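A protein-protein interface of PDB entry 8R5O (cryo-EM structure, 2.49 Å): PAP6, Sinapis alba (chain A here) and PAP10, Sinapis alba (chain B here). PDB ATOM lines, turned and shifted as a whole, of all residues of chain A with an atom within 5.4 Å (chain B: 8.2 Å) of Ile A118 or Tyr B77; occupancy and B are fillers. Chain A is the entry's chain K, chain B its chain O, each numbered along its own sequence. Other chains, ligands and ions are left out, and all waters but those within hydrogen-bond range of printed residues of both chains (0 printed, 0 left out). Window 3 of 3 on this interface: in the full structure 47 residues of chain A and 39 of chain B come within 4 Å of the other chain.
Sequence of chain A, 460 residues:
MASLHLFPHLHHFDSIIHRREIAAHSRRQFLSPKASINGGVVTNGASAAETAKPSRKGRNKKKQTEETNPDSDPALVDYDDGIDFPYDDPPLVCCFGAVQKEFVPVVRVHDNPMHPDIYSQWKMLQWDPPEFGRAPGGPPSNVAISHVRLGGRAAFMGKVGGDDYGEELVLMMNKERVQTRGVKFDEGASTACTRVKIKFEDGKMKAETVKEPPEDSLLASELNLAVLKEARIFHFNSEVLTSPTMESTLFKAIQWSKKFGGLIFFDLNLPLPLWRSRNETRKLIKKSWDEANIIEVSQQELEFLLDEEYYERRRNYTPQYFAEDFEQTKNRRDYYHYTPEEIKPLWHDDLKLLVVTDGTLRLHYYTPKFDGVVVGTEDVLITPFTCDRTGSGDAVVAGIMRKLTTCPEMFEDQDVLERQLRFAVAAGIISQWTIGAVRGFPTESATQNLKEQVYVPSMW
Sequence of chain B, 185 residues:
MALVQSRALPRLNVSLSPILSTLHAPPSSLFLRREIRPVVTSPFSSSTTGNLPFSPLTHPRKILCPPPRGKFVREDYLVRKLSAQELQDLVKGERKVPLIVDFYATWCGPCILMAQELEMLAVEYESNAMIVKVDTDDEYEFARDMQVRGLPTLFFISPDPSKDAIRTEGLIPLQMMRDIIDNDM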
ATOM      1  N   HIS A 115       3.886   3.813  26.189  1.00  0.00           N
ATOM      2  CA  HIS A 115       4.081   2.580  25.441  1.00  0.00           C
ATOM      3  C   HIS A 115       3.009   2.450  24.360  1.00  0.00           C
ATOM      4  O   HIS A 115       1.827   2.699  24.624  1.00  0.00           O
ATOM      5  CB  HIS A 115       4.038   1.370  26.373  1.00  0.00           C
ATOM      6  CG  HIS A 115       4.531   0.106  25.743  1.00  0.00           C
ATOM      7  ND1 HIS A 115       3.728  -0.703  24.968  1.00  0.00           N
ATOM      8  CD2 HIS A 115       5.748  -0.487  25.768  1.00  0.00           C
ATOM      9  CE1 HIS A 115       4.428  -1.740  24.545  1.00  0.00           C
ATOM     10  NE2 HIS A 115       5.656  -1.632  25.016  1.00  0.00           N
ATOM     11  N   PRO A 116       3.387   2.076  23.134  1.00  0.00           N
ATOM     12  CA  PRO A 116       2.399   2.018  22.044  1.00  0.00           C
ATOM     13  C   PRO A 116       1.319   0.965  22.231  1.00  0.00           C
ATOM     14  O   PRO A 116       0.256   1.084  21.609  1.00  0.00           O
ATOM     15  CB  PRO A 116       3.260   1.717  20.809  1.00  0.00           C
ATOM     16  CG  PRO A 116       4.479   1.062  21.351  1.00  0.00           C
ATOM     17  CD  PRO A 116       4.736   1.707  22.680  1.00  0.00           C
ATOM     18  N   ASP A 117       1.546  -0.055  23.054  1.00  0.00           N
ATOM     19  CA  ASP A 117       0.597  -1.151  23.219  1.00  0.00           C
ATOM     20  C   ASP A 117      -0.049  -1.198  24.593  1.00  0.00           C
ATOM     21  O   ASP A 117      -1.236  -1.506  24.699  1.00  0.00           O
ATOM     22  CB  ASP A 117       1.289  -2.493  22.954  1.00  0.00           C
ATOM     23  CG  ASP A 117       1.926  -2.561  21.584  1.00  0.00           C
ATOM     24  OD1 ASP A 117       1.395  -1.936  20.643  1.00  0.00           O
ATOM     25  OD2 ASP A 117       2.963  -3.242  21.446  1.00  0.00           O
ATOM     26  N   ILE A 118       0.702  -0.896  25.647  1.00  0.00           N
ATOM     27  CA  ILE A 118       0.198  -1.004  27.010  1.00  0.00           C
ATOM     28  C   ILE A 118      -0.590   0.253  27.349  1.00  0.00           C
ATOM     29  O   ILE A 118      -0.034   1.230  27.859  1.00  0.00           O
ATOM     30  CB  ILE A 118       1.351  -1.232  28.004  1.00  0.00           C
ATOM     31  CG1 ILE A 118       2.242  -2.378  27.520  1.00  0.00           C
ATOM     32  CG2 ILE A 118       0.813  -1.535  29.388  1.00  0.00           C
ATOM     33  CD1 ILE A 118       3.475  -2.595  28.364  1.00  0.00           C
ATOM     34  N   TYR A 119      -1.894   0.234  27.064  1.00  0.00           N
ATOM     35  CA  TYR A 119      -2.736   1.402  27.292  1.00  0.00           C
ATOM     36  C   TYR A 119      -2.990   1.673  28.768  1.00  0.00           C
ATOM     37  O   TYR A 119      -3.555   2.722  29.094  1.00  0.00           O
ATOM     38  CB  TYR A 119      -4.068   1.247  26.555  1.00  0.00           C
ATOM     39  CG  TYR A 119      -4.716  -0.107  26.717  1.00  0.00           C
ATOM     40  CD1 TYR A 119      -5.391  -0.441  27.882  1.00  0.00           C
ATOM     41  CD2 TYR A 119      -4.660  -1.049  25.701  1.00  0.00           C
ATOM     42  CE1 TYR A 119      -5.985  -1.677  28.033  1.00  0.00           C
ATOM     43  CE2 TYR A 119      -5.251  -2.288  25.843  1.00  0.00           C
ATOM     44  CZ  TYR A 119      -5.912  -2.597  27.011  1.00  0.00           C
ATOM     45  OH  TYR A 119      -6.503  -3.829  27.157  1.00  0.00           O
ATOM     46  N   SER A 120      -2.604   0.763  29.664  1.00  0.00           N
ATOM     47  CA  SER A 120      -2.719   1.041  31.090  1.00  0.00           C
ATOM     48  C   SER A 120      -1.762   2.137  31.539  1.00  0.00           C
ATOM     49  O   SER A 120      -1.984   2.741  32.592  1.00  0.00           O
ATOM     50  CB  SER A 120      -2.476  -0.231  31.904  1.00  0.00           C
ATOM     51  OG  SER A 120      -1.119  -0.632  31.844  1.00  0.00           O
ATOM     52  N   GLN A 121      -0.705   2.401  30.771  1.00  0.00           N
ATOM     53  CA  GLN A 121       0.192   3.511  31.067  1.00  0.00           C
ATOM     54  C   GLN A 121      -0.346   4.846  30.574  1.00  0.00           C
ATOM     55  O   GLN A 121       0.153   5.893  31.000  1.00  0.00           O
ATOM     56  CB  GLN A 121       1.565   3.276  30.435  1.00  0.00           C
ATOM     57  CG  GLN A 121       2.254   1.990  30.842  1.00  0.00           C
ATOM     58  CD  GLN A 121       3.591   1.816  30.149  1.00  0.00           C
ATOM     59  OE1 GLN A 121       4.024   2.680  29.389  1.00  0.00           O
ATOM     60  NE2 GLN A 121       4.251   0.695  30.406  1.00  0.00           N
ATOM     61  N   TRP A 122      -1.343   4.834  29.688  1.00  0.00           N
ATOM     62  CA  TRP A 122      -1.766   6.059  29.022  1.00  0.00           C
ATOM     63  C   TRP A 122      -2.480   7.020  29.962  1.00  0.00           C
ATOM     64  O   TRP A 122      -2.567   8.212  29.654  1.00  0.00           O
ATOM     65  CB  TRP A 122      -2.655   5.723  27.821  1.00  0.00           C
ATOM     66  CG  TRP A 122      -1.951   4.914  26.762  1.00  0.00           C
ATOM     67  CD1 TRP A 122      -0.658   4.476  26.790  1.00  0.00           C
ATOM     68  CD2 TRP A 122      -2.501   4.448  25.524  1.00  0.00           C
ATOM     69  NE1 TRP A 122      -0.370   3.768  25.652  1.00  0.00           N
ATOM     70  CE2 TRP A 122      -1.484   3.734  24.858  1.00  0.00           C
ATOM     71  CE3 TRP A 122      -3.753   4.562  24.916  1.00  0.00           C
ATOM     72  CZ2 TRP A 122      -1.682   3.141  23.614  1.00  0.00           C
ATOM     73  CZ3 TRP A 122      -3.946   3.972  23.682  1.00  0.00           C
ATOM     74  CH2 TRP A 122      -2.917   3.270  23.044  1.00  0.00           C
ATOM     75  N   ARG B  74       2.641 -16.578  24.535  1.00  0.00           N
ATOM     76  CA  ARG B  74       1.870 -15.868  23.525  1.00  0.00           C
ATOM     77  C   ARG B  74       1.917 -14.366  23.780  1.00  0.00           C
ATOM     78  O   ARG B  74       1.849 -13.913  24.927  1.00  0.00           O
ATOM     79  CB  ARG B  74       0.427 -16.369  23.527  1.00  0.00           C
ATOM     80  CG  ARG B  74      -0.492 -15.698  22.525  1.00  0.00           C
ATOM     81  CD  ARG B  74      -0.036 -15.934  21.097  1.00  0.00           C
ATOM     82  NE  ARG B  74      -1.079 -15.597  20.137  1.00  0.00           N
ATOM     83  CZ  ARG B  74      -0.887 -15.463  18.833  1.00  0.00           C
ATOM     84  NH1 ARG B  74       0.311 -15.607  18.293  1.00  0.00           N
ATOM     85  NH2 ARG B  74      -1.923 -15.173  18.051  1.00  0.00           N
ATOM     86  N   GLU B  75       2.045 -13.591  22.708  1.00  0.00           N
ATOM     87  CA  GLU B  75       2.091 -12.143  22.849  1.00  0.00           C
ATOM     88  C   GLU B  75       0.731 -11.607  23.287  1.00  0.00           C
ATOM     89  O   GLU B  75      -0.319 -12.179  22.979  1.00  0.00           O
ATOM     90  CB  GLU B  75       2.531 -11.483  21.540  1.00  0.00           C
ATOM     91  CG  GLU B  75       1.411 -11.215  20.551  1.00  0.00           C
ATOM     92  CD  GLU B  75       0.883 -12.475  19.903  1.00  0.00           C
ATOM     93  OE1 GLU B  75       1.671 -13.422  19.709  1.00  0.00           O
ATOM     94  OE2 GLU B  75      -0.325 -12.518  19.585  1.00  0.00           O
ATOM     95  N   ASP B  76       0.761 -10.501  24.029  1.00  0.00           N
ATOM     96  CA  ASP B  76      -0.445  -9.952  24.633  1.00  0.00           C
ATOM     97  C   ASP B  76      -1.235  -9.042  23.705  1.00  0.00           C
ATOM     98  O   ASP B  76      -2.377  -8.700  24.031  1.00  0.00           O
ATOM     99  CB  ASP B  76      -0.086  -9.185  25.909  1.00  0.00           C
ATOM    100  CG  ASP B  76       0.099 -10.097  27.105  1.00  0.00           C
ATOM    101  OD1 ASP B  76      -0.763 -10.972  27.320  1.00  0.00           O
ATOM    102  OD2 ASP B  76       1.104  -9.938  27.829  1.00  0.00           O
ATOM    103  N   TYR B  77      -0.675  -8.642  22.565  1.00  0.00           N
ATOM    104  CA  TYR B  77      -1.325  -7.667  21.698  1.00  0.00           C
ATOM    105  C   TYR B  77      -1.213  -8.099  20.247  1.00  0.00           C
ATOM    106  O   TYR B  77      -0.123  -8.435  19.775  1.00  0.00           O
ATOM    107  CB  TYR B  77      -0.717  -6.274  21.895  1.00  0.00           C
ATOM    108  CG  TYR B  77      -0.920  -5.745  23.293  1.00  0.00           C
ATOM    109  CD1 TYR B  77      -2.121  -5.154  23.662  1.00  0.00           C
ATOM    110  CD2 TYR B  77       0.079  -5.851  24.251  1.00  0.00           C
ATOM    111  CE1 TYR B  77      -2.318  -4.677  24.941  1.00  0.00           C
ATOM    112  CE2 TYR B  77      -0.109  -5.374  25.531  1.00  0.00           C
ATOM    113  CZ  TYR B  77      -1.310  -4.789  25.871  1.00  0.00           C
ATOM    114  OH  TYR B  77      -1.504  -4.312  27.145  1.00  0.00           O
ATOM    115  N   LEU B  78      -2.343  -8.074  19.540  1.00  0.00           N
ATOM    116  CA  LEU B  78      -2.409  -8.537  18.160  1.00  0.00           C
ATOM    117  C   LEU B  78      -2.266  -7.414  17.141  1.00  0.00           C
ATOM    118  O   LEU B  78      -1.758  -7.654  16.041  1.00  0.00           O
ATOM    119  CB  LEU B  78      -3.729  -9.274  17.914  1.00  0.00           C
ATOM    120  CG  LEU B  78      -3.816 -10.775  18.216  1.00  0.00           C
ATOM    121  CD1 LEU B  78      -3.395 -11.094  19.639  1.00  0.00           C
ATOM    122  CD2 LEU B  78      -5.226 -11.277  17.957  1.00  0.00           C
ATOM    123  N   VAL B  79      -2.701  -6.202  17.472  1.00  0.00           N
ATOM    124  CA  VAL B  79      -2.687  -5.099  16.516  1.00  0.00           C
ATOM    125  C   VAL B  79      -1.266  -4.561  16.401  1.00  0.00           C
ATOM    126  O   VAL B  79      -0.645  -4.196  17.406  1.00  0.00           O
ATOM    127  CB  VAL B  79      -3.667  -3.993  16.931  1.00  0.00           C
ATOM    128  CG1 VAL B  79      -3.604  -2.833  15.951  1.00  0.00           C
ATOM    129  CG2 VAL B  79      -5.080  -4.544  17.019  1.00  0.00           C
ATOM    130  N   ARG B  80      -0.750  -4.508  15.177  1.00  0.00           N
ATOM    131  CA  ARG B  80       0.604  -4.038  14.924  1.00  0.00           C
ATOM    132  C   ARG B  80       0.623  -2.539  14.667  1.00  0.00           C
ATOM    133  O   ARG B  80      -0.290  -1.987  14.048  1.00  0.00           O
ATOM    134  CB  ARG B  80       1.219  -4.762  13.726  1.00  0.00           C
ATOM    135  CG  ARG B  80       1.672  -6.181  13.997  1.00  0.00           C
ATOM    136  CD  ARG B  80       2.751  -6.569  13.005  1.00  0.00           C
ATOM    137  NE  ARG B  80       2.372  -6.216  11.641  1.00  0.00           N
ATOM    138  CZ  ARG B  80       3.226  -6.083  10.635  1.00  0.00           C
ATOM    139  NH1 ARG B  80       4.528  -6.246  10.808  1.00  0.00           N
ATOM    140  NH2 ARG B  80       2.762  -5.770   9.429  1.00  0.00           N
ATOM    141  N   TYR B 104      -4.209   6.802  16.245  1.00  0.00           N
ATOM    142  CA  TYR B 104      -4.375   6.970  17.680  1.00  0.00           C
ATOM    143  C   TYR B 104      -3.221   7.794  18.228  1.00  0.00           C
ATOM    144  O   TYR B 104      -2.234   8.062  17.539  1.00  0.00           O
ATOM    145  CB  TYR B 104      -4.457   5.617  18.394  1.00  0.00           C
ATOM    146  CG  TYR B 104      -3.118   4.940  18.587  1.00  0.00           C
ATOM    147  CD1 TYR B 104      -2.429   4.395  17.513  1.00  0.00           C
ATOM    148  CD2 TYR B 104      -2.545   4.841  19.848  1.00  0.00           C
ATOM    149  CE1 TYR B 104      -1.206   3.777  17.686  1.00  0.00           C
ATOM    150  CE2 TYR B 104      -1.324   4.225  20.031  1.00  0.00           C
ATOM    151  CZ  TYR B 104      -0.659   3.694  18.948  1.00  0.00           C
ATOM    152  OH  TYR B 104       0.556   3.078  19.130  1.00  0.00           O
ATOM    153  N   THR B 106      -1.303   8.234  22.338  1.00  0.00           N
ATOM    154  CA  THR B 106      -1.327   7.756  23.716  1.00  0.00           C
ATOM    155  C   THR B 106      -1.867   8.794  24.692  1.00  0.00           C
ATOM    156  O   THR B 106      -2.263   8.430  25.803  1.00  0.00           O
ATOM    157  CB  THR B 106       0.072   7.317  24.148  1.00  0.00           C
ATOM    158  OG1 THR B 106       0.996   8.399  23.978  1.00  0.00           O
ATOM    159  CG2 THR B 106       0.532   6.123  23.323  1.00  0.00           C
ATOM    160  N   ILE B 112      -7.843   4.930  24.474  1.00  0.00           N
ATOM    161  CA  ILE B 112      -7.762   3.786  25.379  1.00  0.00           C
ATOM    162  C   ILE B 112      -8.940   2.847  25.151  1.00  0.00           C
ATOM    163  O   ILE B 112      -8.780   1.622  25.118  1.00  0.00           O
ATOM    164  CB  ILE B 112      -7.694   4.265  26.841  1.00  0.00           C
ATOM    165  CG1 ILE B 112      -6.488   5.180  27.044  1.00  0.00           C
ATOM    166  CG2 ILE B 112      -7.636   3.080  27.792  1.00  0.00           C
ATOM    167  CD1 ILE B 112      -6.397   5.769  28.430  1.00  0.00           C
ATOM    168  N   ALA B 115      -8.567   1.179  21.647  1.00  0.00           N
ATOM    169  CA  ALA B 115      -7.528   0.156  21.583  1.00  0.00           C
ATOM    170  C   ALA B 115      -8.057  -1.202  22.022  1.00  0.00           C
ATOM    171  O   ALA B 115      -7.692  -2.234  21.445  1.00  0.00           O
ATOM    172  CB  ALA B 115      -6.331   0.568  22.441  1.00  0.00           C
ATOM    173  N   GLN B 116      -8.919  -1.225  23.041  1.00  0.00           N
ATOM    174  CA  GLN B 116      -9.467  -2.490  23.514  1.00  0.00           C
ATOM    175  C   GLN B 116     -10.468  -3.083  22.531  1.00  0.00           C
ATOM    176  O   GLN B 116     -10.580  -4.310  22.429  1.00  0.00           O
ATOM    177  CB  GLN B 116     -10.116  -2.300  24.884  1.00  0.00           C
ATOM    178  CG  GLN B 116      -9.142  -1.911  25.978  1.00  0.00           C
ATOM    179  CD  GLN B 116      -9.834  -1.618  27.291  1.00  0.00           C
ATOM    180  OE1 GLN B 116      -9.972  -2.496  28.142  1.00  0.00           O
ATOM    181  NE2 GLN B 116     -10.272  -0.377  27.464  1.00  0.00           N
ATOM    182  N   GLU B 119      -8.437  -4.742  19.576  1.00  0.00           N
ATOM    183  CA  GLU B 119      -7.846  -6.016  19.972  1.00  0.00           C
ATOM    184  C   GLU B 119      -8.886  -7.126  19.949  1.00  0.00           C
ATOM    185  O   GLU B 119      -8.596  -8.253  19.531  1.00  0.00           O
ATOM    186  CB  GLU B 119      -7.209  -5.899  21.356  1.00  0.00           C
ATOM    187  CG  GLU B 119      -5.923  -5.087  21.390  1.00  0.00           C
ATOM    188  CD  GLU B 119      -4.765  -5.785  20.697  1.00  0.00           C
ATOM    189  OE1 GLU B 119      -4.829  -7.018  20.511  1.00  0.00           O
ATOM    190  OE2 GLU B 119      -3.785  -5.097  20.341  1.00  0.00           O
ATOM    191  N   ALA B 122      -9.526  -8.006  16.367  1.00  0.00           N
ATOM    192  CA  ALA B 122      -8.468  -8.847  15.817  1.00  0.00           C
ATOM    193  C   ALA B 122      -8.663 -10.307  16.207  1.00  0.00           C
ATOM    194  O   ALA B 122      -8.344 -11.210  15.427  1.00  0.00           O
ATOM    195  CB  ALA B 122      -7.104  -8.341  16.282  1.00  0.00           C
ATOM    196  N   VAL B 123      -9.169 -10.559  17.416  1.00  0.00           N
ATOM    197  CA  VAL B 123      -9.434 -11.930  17.839  1.00  0.00           C
ATOM    198  C   VAL B 123     -10.559 -12.538  17.009  1.00  0.00           C
ATOM    199  O   VAL B 123     -10.475 -13.695  16.582  1.00  0.00           O
ATOM    200  CB  VAL B 123      -9.747 -11.976  19.344  1.00  0.00           C
ATOM    201  CG1 VAL B 123     -10.138 -13.383  19.765  1.00  0.00           C
ATOM    202  CG2 VAL B 123      -8.555 -11.492  20.149  1.00  0.00           C
ATOM    203  N   LYS B 133      -2.303  -0.119  13.261  1.00  0.00           N
ATOM    204  CA  LYS B 133      -2.483   1.168  13.913  1.00  0.00           C
ATOM    205  C   LYS B 133      -1.301   2.075  13.601  1.00  0.00           C
ATOM    206  O   LYS B 133      -0.180   1.608  13.388  1.00  0.00           O
ATOM    207  CB  LYS B 133      -2.652   1.014  15.432  1.00  0.00           C
ATOM    208  CG  LYS B 133      -1.495   0.327  16.129  1.00  0.00           C
ATOM    209  CD  LYS B 133      -1.801   0.097  17.595  1.00  0.00           C
ATOM    210  CE  LYS B 133      -0.637  -0.567  18.304  1.00  0.00           C
ATOM    211  NZ  LYS B 133      -0.958  -0.870  19.722  1.00  0.00           N
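Ile A118 touches just one residue of chain B: Tyr B77.
Printed residues of chain A within 4 Å of Ile B112: Trp A122.
Of the printed residues of chain B, Trp A122 touches Tyr B104 (3.5 Å), Thr B106 (3.4 Å) and Ile B112 (3.5 Å).
Of the printed residues of chain B, Pro A116 touches Tyr B104 and Lys B133.
Of the printed residues of chain A, Gln B116 touches Tyr A119 (3.5 Å).
The nearest printed residue of chain A that does not touch Tyr B77 is Ser A120 (5.8 Å).
O of Pro A116 lies within hydrogen-bond range of OH of Tyr B104, 3.2 Å away.
The backbone carbonyl oxygen (O) of Pro A116 sits at hydrogen-bond distance from the side-chain amino group (NZ) of Lys B133, at 3.0 Å.
The side-chain amino group (NZ) of Lys B133 lies within salt-bridge range of the side-chain carboxylate (OD1) of Asp A117 (2.7 Å).
Of the 16 printed residues of chain B, 6 touch a printed residue of chain A.
Printed residues of chain B that touch a printed residue of chain A: Tyr B77, Tyr B104, Thr B106, Ile B112, Gln B116 and Lys B133.
Along chain B the printed residues that touch a printed residue of chain A span positions 77 to 133.
Of the 8 printed residues of chain A, 6 touch a printed residue of chain B.
Printed residues of chain A that touch a printed residue of chain B: His A115, Pro A116, Asp A117, Ile A118, Tyr A119 and Trp A122.
Hydrophobic or aromatic side chains of chain A within 4 Å of the printed part of chain B: Pro A116, Tyr A119 and Trp A122.
Among the printed residues, 11 pairs touch across the chains.
Among the printed residues, merely in contact across the chains: His A115 with Thr B106 (3.9 Å), Asp A117 with Tyr B77 (3.4 Å), Ile A118 with Tyr B77 (3.7 Å), Tyr A119 with Tyr B77 (3.9 Å), Tyr A119 with Gln B116 (3.5 Å), Trp A122 with Tyr B104 (3.5 Å), Trp A122 with Thr B106 (3.4 Å) and Trp A122 with Ile B112 (3.5 Å).
The backbone NH (N) of Asp A117 sits at hydrogen-bond distance from a ring nitrogen (ND1) of His A115, 3.0 Å away.
OE1 of Gln A121 lies close to N of His A115 (3.4 Å).
The backbone carbonyl oxygen (O) of His A115 is in hydrogen-bond range of the indole nitrogen (NE1) of Trp A122.
The indole nitrogen (NE1) of Trp A122 is in hydrogen-bond range of the backbone carbonyl oxygen (O) of Ile A118 (3.4 Å).
The backbone carbonyl oxygen of Arg B80 sits at hydrogen-bond distance from the backbone NH of Lys B133, 2.9 Å away.
The backbone carbonyl oxygen (O) of Ile B112 is in hydrogen-bond range of the side-chain amide nitrogen (NE2) of Gln B116 (3.4 Å).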
